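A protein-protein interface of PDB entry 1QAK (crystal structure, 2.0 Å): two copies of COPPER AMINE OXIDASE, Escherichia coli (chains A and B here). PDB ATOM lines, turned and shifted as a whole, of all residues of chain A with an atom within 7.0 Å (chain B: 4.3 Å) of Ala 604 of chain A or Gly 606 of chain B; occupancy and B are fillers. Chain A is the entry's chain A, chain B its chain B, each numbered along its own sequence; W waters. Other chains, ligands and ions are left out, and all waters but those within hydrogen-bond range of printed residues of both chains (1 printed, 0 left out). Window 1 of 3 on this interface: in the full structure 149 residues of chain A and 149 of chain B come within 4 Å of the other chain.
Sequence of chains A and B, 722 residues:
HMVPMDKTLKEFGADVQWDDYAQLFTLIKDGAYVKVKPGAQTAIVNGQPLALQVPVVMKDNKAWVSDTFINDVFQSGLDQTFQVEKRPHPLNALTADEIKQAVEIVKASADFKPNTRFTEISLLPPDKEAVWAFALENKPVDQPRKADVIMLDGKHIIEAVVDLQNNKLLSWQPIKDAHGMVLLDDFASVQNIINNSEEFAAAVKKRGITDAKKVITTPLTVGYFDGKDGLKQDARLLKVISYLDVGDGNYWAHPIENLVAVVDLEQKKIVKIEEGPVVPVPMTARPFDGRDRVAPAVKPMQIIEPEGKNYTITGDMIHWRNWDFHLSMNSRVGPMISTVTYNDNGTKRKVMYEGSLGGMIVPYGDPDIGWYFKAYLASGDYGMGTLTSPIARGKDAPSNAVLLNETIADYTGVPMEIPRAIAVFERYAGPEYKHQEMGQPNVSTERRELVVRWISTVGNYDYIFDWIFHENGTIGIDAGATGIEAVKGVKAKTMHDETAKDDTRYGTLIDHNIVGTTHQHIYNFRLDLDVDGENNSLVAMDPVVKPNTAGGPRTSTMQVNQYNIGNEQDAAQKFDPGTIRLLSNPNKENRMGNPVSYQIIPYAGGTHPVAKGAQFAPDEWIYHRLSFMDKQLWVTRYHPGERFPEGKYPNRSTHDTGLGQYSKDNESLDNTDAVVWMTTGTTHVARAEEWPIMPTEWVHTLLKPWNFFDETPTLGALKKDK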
ATOM      1  N   ASP A 478      -8.949  11.786  13.970  1.00  0.00           N
ATOM      2  CA  ASP A 478      -9.645  10.521  14.326  1.00  0.00           C
ATOM      3  C   ASP A 478      -8.935   9.362  13.648  1.00  0.00           C
ATOM      4  O   ASP A 478      -8.300   9.574  12.599  1.00  0.00           O
ATOM      5  CB  ASP A 478     -11.089  10.545  13.815  1.00  0.00           C
ATOM      6  CG  ASP A 478     -12.021  11.408  14.646  1.00  0.00           C
ATOM      7  OD1 ASP A 478     -11.684  12.044  15.652  1.00  0.00           O
ATOM      8  OD2 ASP A 478     -13.220  11.518  14.330  1.00  0.00           O
ATOM      9  N   PHE A 575      -3.592  10.898  30.790  1.00  0.00           N
ATOM     10  CA  PHE A 575      -4.534  11.965  30.490  1.00  0.00           C
ATOM     11  C   PHE A 575      -5.865  11.670  31.167  1.00  0.00           C
ATOM     12  O   PHE A 575      -6.511  10.668  30.879  1.00  0.00           O
ATOM     13  CB  PHE A 575      -4.887  12.081  28.984  1.00  0.00           C
ATOM     14  CG  PHE A 575      -5.850  13.218  28.730  1.00  0.00           C
ATOM     15  CD1 PHE A 575      -5.538  14.536  29.009  1.00  0.00           C
ATOM     16  CD2 PHE A 575      -7.100  12.967  28.189  1.00  0.00           C
ATOM     17  CE1 PHE A 575      -6.420  15.574  28.770  1.00  0.00           C
ATOM     18  CE2 PHE A 575      -7.990  13.999  27.940  1.00  0.00           C
ATOM     19  CZ  PHE A 575      -7.672  15.314  28.236  1.00  0.00           C
ATOM     20  N   PRO A 577      -9.496  12.772  31.262  1.00  0.00           N
ATOM     21  CA  PRO A 577     -10.396  13.541  30.424  1.00  0.00           C
ATOM     22  C   PRO A 577     -11.180  14.603  31.198  1.00  0.00           C
ATOM     23  O   PRO A 577     -11.755  15.484  30.563  1.00  0.00           O
ATOM     24  CB  PRO A 577     -11.275  12.556  29.652  1.00  0.00           C
ATOM     25  CG  PRO A 577     -11.128  11.327  30.498  1.00  0.00           C
ATOM     26  CD  PRO A 577      -9.841  11.344  31.276  1.00  0.00           C
ATOM     27  N   ILE A 601      -6.554  17.349  23.713  1.00  0.00           N
ATOM     28  CA  ILE A 601      -7.391  16.259  24.260  1.00  0.00           C
ATOM     29  C   ILE A 601      -7.041  14.943  23.559  1.00  0.00           C
ATOM     30  O   ILE A 601      -7.577  14.577  22.488  1.00  0.00           O
ATOM     31  CB  ILE A 601      -8.877  16.546  24.021  1.00  0.00           C
ATOM     32  CG1 ILE A 601      -9.223  17.923  24.567  1.00  0.00           C
ATOM     33  CG2 ILE A 601      -9.724  15.501  24.765  1.00  0.00           C
ATOM     34  CD1 ILE A 601     -10.630  18.455  24.405  1.00  0.00           C
ATOM     35  N   PRO A 602      -6.108  14.215  24.149  1.00  0.00           N
ATOM     36  CA  PRO A 602      -5.617  12.932  23.632  1.00  0.00           C
ATOM     37  C   PRO A 602      -6.715  11.876  23.658  1.00  0.00           C
ATOM     38  O   PRO A 602      -6.711  10.844  22.968  1.00  0.00           O
ATOM     39  CB  PRO A 602      -4.485  12.469  24.580  1.00  0.00           C
ATOM     40  CG  PRO A 602      -4.195  13.729  25.347  1.00  0.00           C
ATOM     41  CD  PRO A 602      -5.428  14.601  25.393  1.00  0.00           C
ATOM     42  N   TYR A 603      -7.717  12.145  24.483  1.00  0.00           N
ATOM     43  CA  TYR A 603      -8.805  11.149  24.536  1.00  0.00           C
ATOM     44  C   TYR A 603     -10.145  11.854  24.404  1.00  0.00           C
ATOM     45  O   TYR A 603     -10.564  12.411  25.425  1.00  0.00           O
ATOM     46  CB  TYR A 603      -8.722  10.187  25.731  1.00  0.00           C
ATOM     47  CG  TYR A 603      -9.945   9.283  25.756  1.00  0.00           C
ATOM     48  CD1 TYR A 603     -10.319   8.411  24.756  1.00  0.00           C
ATOM     49  CD2 TYR A 603     -10.756   9.358  26.889  1.00  0.00           C
ATOM     50  CE1 TYR A 603     -11.460   7.628  24.861  1.00  0.00           C
ATOM     51  CE2 TYR A 603     -11.892   8.575  27.009  1.00  0.00           C
ATOM     52  CZ  TYR A 603     -12.242   7.716  25.987  1.00  0.00           C
ATOM     53  OH  TYR A 603     -13.403   6.999  26.214  1.00  0.00           O
ATOM     54  N   ALA A 604     -10.718  11.822  23.198  1.00  0.00           N
ATOM     55  CA  ALA A 604     -12.012  12.508  23.089  1.00  0.00           C
ATOM     56  C   ALA A 604     -13.123  11.505  22.786  1.00  0.00           C
ATOM     57  O   ALA A 604     -14.219  11.848  22.353  1.00  0.00           O
ATOM     58  CB  ALA A 604     -11.877  13.578  22.028  1.00  0.00           C
ATOM     59  N   GLY A 605     -12.832  10.227  23.019  1.00  0.00           N
ATOM     60  CA  GLY A 605     -13.820   9.186  22.779  1.00  0.00           C
ATOM     61  C   GLY A 605     -13.398   8.072  21.838  1.00  0.00           C
ATOM     62  O   GLY A 605     -12.341   8.204  21.205  1.00  0.00           O
ATOM     63  N   GLY A 606     -14.214   7.022  21.797  1.00  0.00           N
ATOM     64  CA  GLY A 606     -13.939   5.877  20.932  1.00  0.00           C
ATOM     65  C   GLY A 606     -15.105   4.892  21.038  1.00  0.00           C
ATOM     66  O   GLY A 606     -15.893   4.955  22.004  1.00  0.00           O
ATOM     67  N   THR A 680      -3.185   7.479  21.903  1.00  0.00           N
ATOM     68  CA  THR A 680      -4.579   7.122  22.163  1.00  0.00           C
ATOM     69  C   THR A 680      -4.701   5.661  21.760  1.00  0.00           C
ATOM     70  O   THR A 680      -4.167   5.234  20.730  1.00  0.00           O
ATOM     71  CB  THR A 680      -5.539   8.048  21.411  1.00  0.00           C
ATOM     72  OG1 THR A 680      -6.852   7.704  21.872  1.00  0.00           O
ATOM     73  CG2 THR A 680      -5.571   7.843  19.916  1.00  0.00           C
ATOM     74  N   VAL A 699     -11.646   6.138  17.065  1.00  0.00           N
ATOM     75  CA  VAL A 699     -11.185   6.778  18.284  1.00  0.00           C
ATOM     76  C   VAL A 699     -11.088   8.262  17.890  1.00  0.00           C
ATOM     77  O   VAL A 699     -10.819   8.628  16.736  1.00  0.00           O
ATOM     78  CB  VAL A 699      -9.891   6.314  18.970  1.00  0.00           C
ATOM     79  CG1 VAL A 699     -10.036   4.856  19.397  1.00  0.00           C
ATOM     80  CG2 VAL A 699      -8.737   6.539  18.011  1.00  0.00           C
ATOM     81  N   HIS A 700     -11.292   9.171  18.818  1.00  0.00           N
ATOM     82  CA  HIS A 700     -11.233  10.596  18.515  1.00  0.00           C
ATOM     83  C   HIS A 700     -10.318  11.382  19.446  1.00  0.00           C
ATOM     84  O   HIS A 700     -10.276  11.042  20.610  1.00  0.00           O
ATOM     85  CB  HIS A 700     -12.640  11.195  18.786  1.00  0.00           C
ATOM     86  CG  HIS A 700     -13.722  10.317  18.240  1.00  0.00           C
ATOM     87  ND1 HIS A 700     -14.069  10.374  16.903  1.00  0.00           N
ATOM     88  CD2 HIS A 700     -14.516   9.381  18.817  1.00  0.00           C
ATOM     89  CE1 HIS A 700     -15.041   9.500  16.699  1.00  0.00           C
ATOM     90  NE2 HIS A 700     -15.336   8.871  17.822  1.00  0.00           N
ATOM     91  N   THR A 701      -9.660  12.373  18.863  1.00  0.00           N
ATOM     92  CA  THR A 701      -8.746  13.240  19.601  1.00  0.00           C
ATOM     93  C   THR A 701      -9.097  14.654  19.129  1.00  0.00           C
ATOM     94  O   THR A 701      -9.707  14.828  18.057  1.00  0.00           O
ATOM     95  CB  THR A 701      -7.260  12.913  19.408  1.00  0.00           C
ATOM     96  OG1 THR A 701      -6.914  13.440  18.147  1.00  0.00           O
ATOM     97  CG2 THR A 701      -6.956  11.414  19.445  1.00  0.00           C
ATOM     98  N   LEU A 702      -8.730  15.661  19.916  1.00  0.00           N
ATOM     99  CA  LEU A 702      -9.036  17.044  19.552  1.00  0.00           C
ATOM    100  C   LEU A 702      -8.049  18.084  20.069  1.00  0.00           C
ATOM    101  O   LEU A 702      -7.431  17.879  21.107  1.00  0.00           O
ATOM    102  CB  LEU A 702     -10.385  17.274  20.222  1.00  0.00           C
ATOM    103  CG  LEU A 702     -11.551  18.029  19.614  1.00  0.00           C
ATOM    104  CD1 LEU A 702     -11.851  17.721  18.154  1.00  0.00           C
ATOM    105  CD2 LEU A 702     -12.777  17.806  20.509  1.00  0.00           C
ATOM    106  N   GLY B 605     -17.100   9.314  24.823  1.00  0.00           N
ATOM    107  CA  GLY B 605     -16.373  10.513  24.421  1.00  0.00           C
ATOM    108  C   GLY B 605     -17.184  11.807  24.436  1.00  0.00           C
ATOM    109  O   GLY B 605     -18.409  11.803  24.604  1.00  0.00           O
ATOM    110  N   GLY B 606     -16.497  12.925  24.267  1.00  0.00           N
ATOM    111  CA  GLY B 606     -17.098  14.245  24.255  1.00  0.00           C
ATOM    112  C   GLY B 606     -16.080  15.326  23.861  1.00  0.00           C
ATOM    113  O   GLY B 606     -14.867  15.078  23.845  1.00  0.00           O
ATOM    114  N   THR B 607     -16.609  16.526  23.586  1.00  0.00           N
ATOM    115  CA  THR B 607     -15.705  17.609  23.187  1.00  0.00           C
ATOM    116  C   THR B 607     -15.431  18.589  24.311  1.00  0.00           C
ATOM    117  O   THR B 607     -14.642  19.505  24.085  1.00  0.00           O
ATOM    118  CB  THR B 607     -16.235  18.331  21.928  1.00  0.00           C
ATOM    119  OG1 THR B 607     -17.546  18.855  22.250  1.00  0.00           O
ATOM    120  CG2 THR B 607     -16.419  17.315  20.796  1.00  0.00           C
ATOM    121  N   HIS B 608     -16.035  18.434  25.487  1.00  0.00           N
ATOM    122  CA  HIS B 608     -15.801  19.311  26.637  1.00  0.00           C
ATOM    123  C   HIS B 608     -15.177  18.341  27.646  1.00  0.00           C
ATOM    124  O   HIS B 608     -15.269  17.102  27.523  1.00  0.00           O
ATOM    125  CB  HIS B 608     -17.097  19.839  27.294  1.00  0.00           C
ATOM    126  CG  HIS B 608     -17.492  21.254  26.988  1.00  0.00           C
ATOM    127  ND1 HIS B 608     -16.615  22.197  26.505  1.00  0.00           N
ATOM    128  CD2 HIS B 608     -18.646  21.931  27.059  1.00  0.00           C
ATOM    129  CE1 HIS B 608     -17.174  23.378  26.287  1.00  0.00           C
ATOM    130  NE2 HIS B 608     -18.441  23.224  26.632  1.00  0.00           N
ATOM    131  N   TRP B 698     -20.396  18.326  21.830  1.00  0.00           N
ATOM    132  CA  TRP B 698     -21.140  17.060  21.923  1.00  0.00           C
ATOM    133  C   TRP B 698     -20.575  16.012  22.852  1.00  0.00           C
ATOM    134  O   TRP B 698     -19.359  16.062  23.049  1.00  0.00           O
ATOM    135  CB  TRP B 698     -20.946  16.426  20.509  1.00  0.00           C
ATOM    136  CG  TRP B 698     -21.756  17.092  19.425  1.00  0.00           C
ATOM    137  CD1 TRP B 698     -21.317  18.052  18.552  1.00  0.00           C
ATOM    138  CD2 TRP B 698     -23.135  16.856  19.094  1.00  0.00           C
ATOM    139  NE1 TRP B 698     -22.326  18.424  17.693  1.00  0.00           N
ATOM    140  CE2 TRP B 698     -23.455  17.700  18.004  1.00  0.00           C
ATOM    141  CE3 TRP B 698     -24.119  15.996  19.598  1.00  0.00           C
ATOM    142  CZ2 TRP B 698     -24.720  17.742  17.434  1.00  0.00           C
ATOM    143  CZ3 TRP B 698     -25.398  16.003  19.041  1.00  0.00           C
ATOM    144  CH2 TRP B 698     -25.654  16.889  17.972  1.00  0.00           C
ATOM    145  N   VAL B 699     -21.444  15.129  23.360  1.00  0.00           N
ATOM    146  CA  VAL B 699     -21.083  14.019  24.190  1.00  0.00           C
ATOM    147  C   VAL B 699     -21.648  12.785  23.453  1.00  0.00           C
ATOM    148  O   VAL B 699     -22.710  12.900  22.827  1.00  0.00           O
ATOM    149  CB  VAL B 699     -21.394  13.914  25.686  1.00  0.00           C
ATOM    150  CG1 VAL B 699     -20.649  15.039  26.401  1.00  0.00           C
ATOM    151  CG2 VAL B 699     -22.883  14.097  25.926  1.00  0.00           C
ATOM    152  N   HIS B 700     -21.003  11.641  23.516  1.00  0.00           N
ATOM    153  CA  HIS B 700     -21.449  10.425  22.834  1.00  0.00           C
ATOM    154  C   HIS B 700     -21.585   9.232  23.781  1.00  0.00           C
ATOM    155  O   HIS B 700     -20.780   9.067  24.684  1.00  0.00           O
ATOM    156  CB  HIS B 700     -20.390   9.985  21.787  1.00  0.00           C
ATOM    157  CG  HIS B 700     -19.885  11.165  21.020  1.00  0.00           C
ATOM    158  ND1 HIS B 700     -20.607  11.775  20.017  1.00  0.00           N
ATOM    159  CD2 HIS B 700     -18.714  11.855  21.139  1.00  0.00           C
ATOM    160  CE1 HIS B 700     -19.884  12.791  19.561  1.00  0.00           C
ATOM    161  NE2 HIS B 700     -18.743  12.865  20.216  1.00  0.00           N
HETATM  162  O   HOH W   1     -15.614  13.428  20.502  1.00  0.00           O
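Gly 605 of chain B touches its own counterpart, Gly 605 of chain A. Positions printed for both chains: 605, 606, 699 and 700.
Of the 14 printed residues of chain A, 3 touch a printed residue of chain B. Along chain A the printed residues that touch a printed residue of chain B span positions 604 to 702. Of the 7 printed residues of chain B, 3 touch a printed residue of chain A. Along chain B the printed residues that touch a printed residue of chain A span positions 605 to 607. Among the printed residues, no Asp or Glu carboxylate lies within 4 Å of a Lys or Arg side-chain nitrogen of the other chain.
N of Ile 601 of chain A is in hydrogen-bond range of O of Leu 702 of chain A (2.8 Å). O of Gly 605 of chain B lies within hydrogen-bond range of N of His 700 of chain B. The backbone NH (N) of Thr 607 of chain B is in hydrogen-bond range of the backbone carbonyl oxygen (O) of Trp 698 of chain B. The backbone NH (N) of Ala 604 of chain A is in hydrogen-bond range of the backbone carbonyl oxygen (O) of His 700 of chain A (2.7 Å). The backbone NH (N) of His 700 of chain A sits at hydrogen-bond distance from the backbone carbonyl oxygen (O) of Gly 605 of chain A (2.8 Å).
Of chain B, only Gly 605 (3.3 Å) and Gly 606 (3.2 Å) come within 4 Å of Ala 604 of chain A. Printed residues of chain B within 4 Å of Gly 605 of chain A: Gly 605 (3.3 Å). Printed residues of chain A within 4 Å of Gly 606 of chain B: Ala 604. Of the printed residues of chain A, Thr 607 of chain B touches Leu 702. Val 699 of chain B touches none of the printed residues of chain A.
The backbone carbonyl oxygen (O) of Ala 604 of chain A is in hydrogen-bond range of the backbone NH (N) of Gly 606 of chain B (3.2 Å).
Among the printed residues, pairs that only touch across the chains: Ala 604 of chain A with Gly 605 of chain B (3.3 Å), Gly 605 of chain A with Gly 605 of chain B (3.3 Å) and Leu 702 of chain A with Thr 607 of chain B (3.7 Å).
Water W1 bridges the backbone carbonyl oxygen of Ala 604 of chain A (2.8 Å) and a ring nitrogen (NE2) of His 700 of chain B (3.2 Å).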
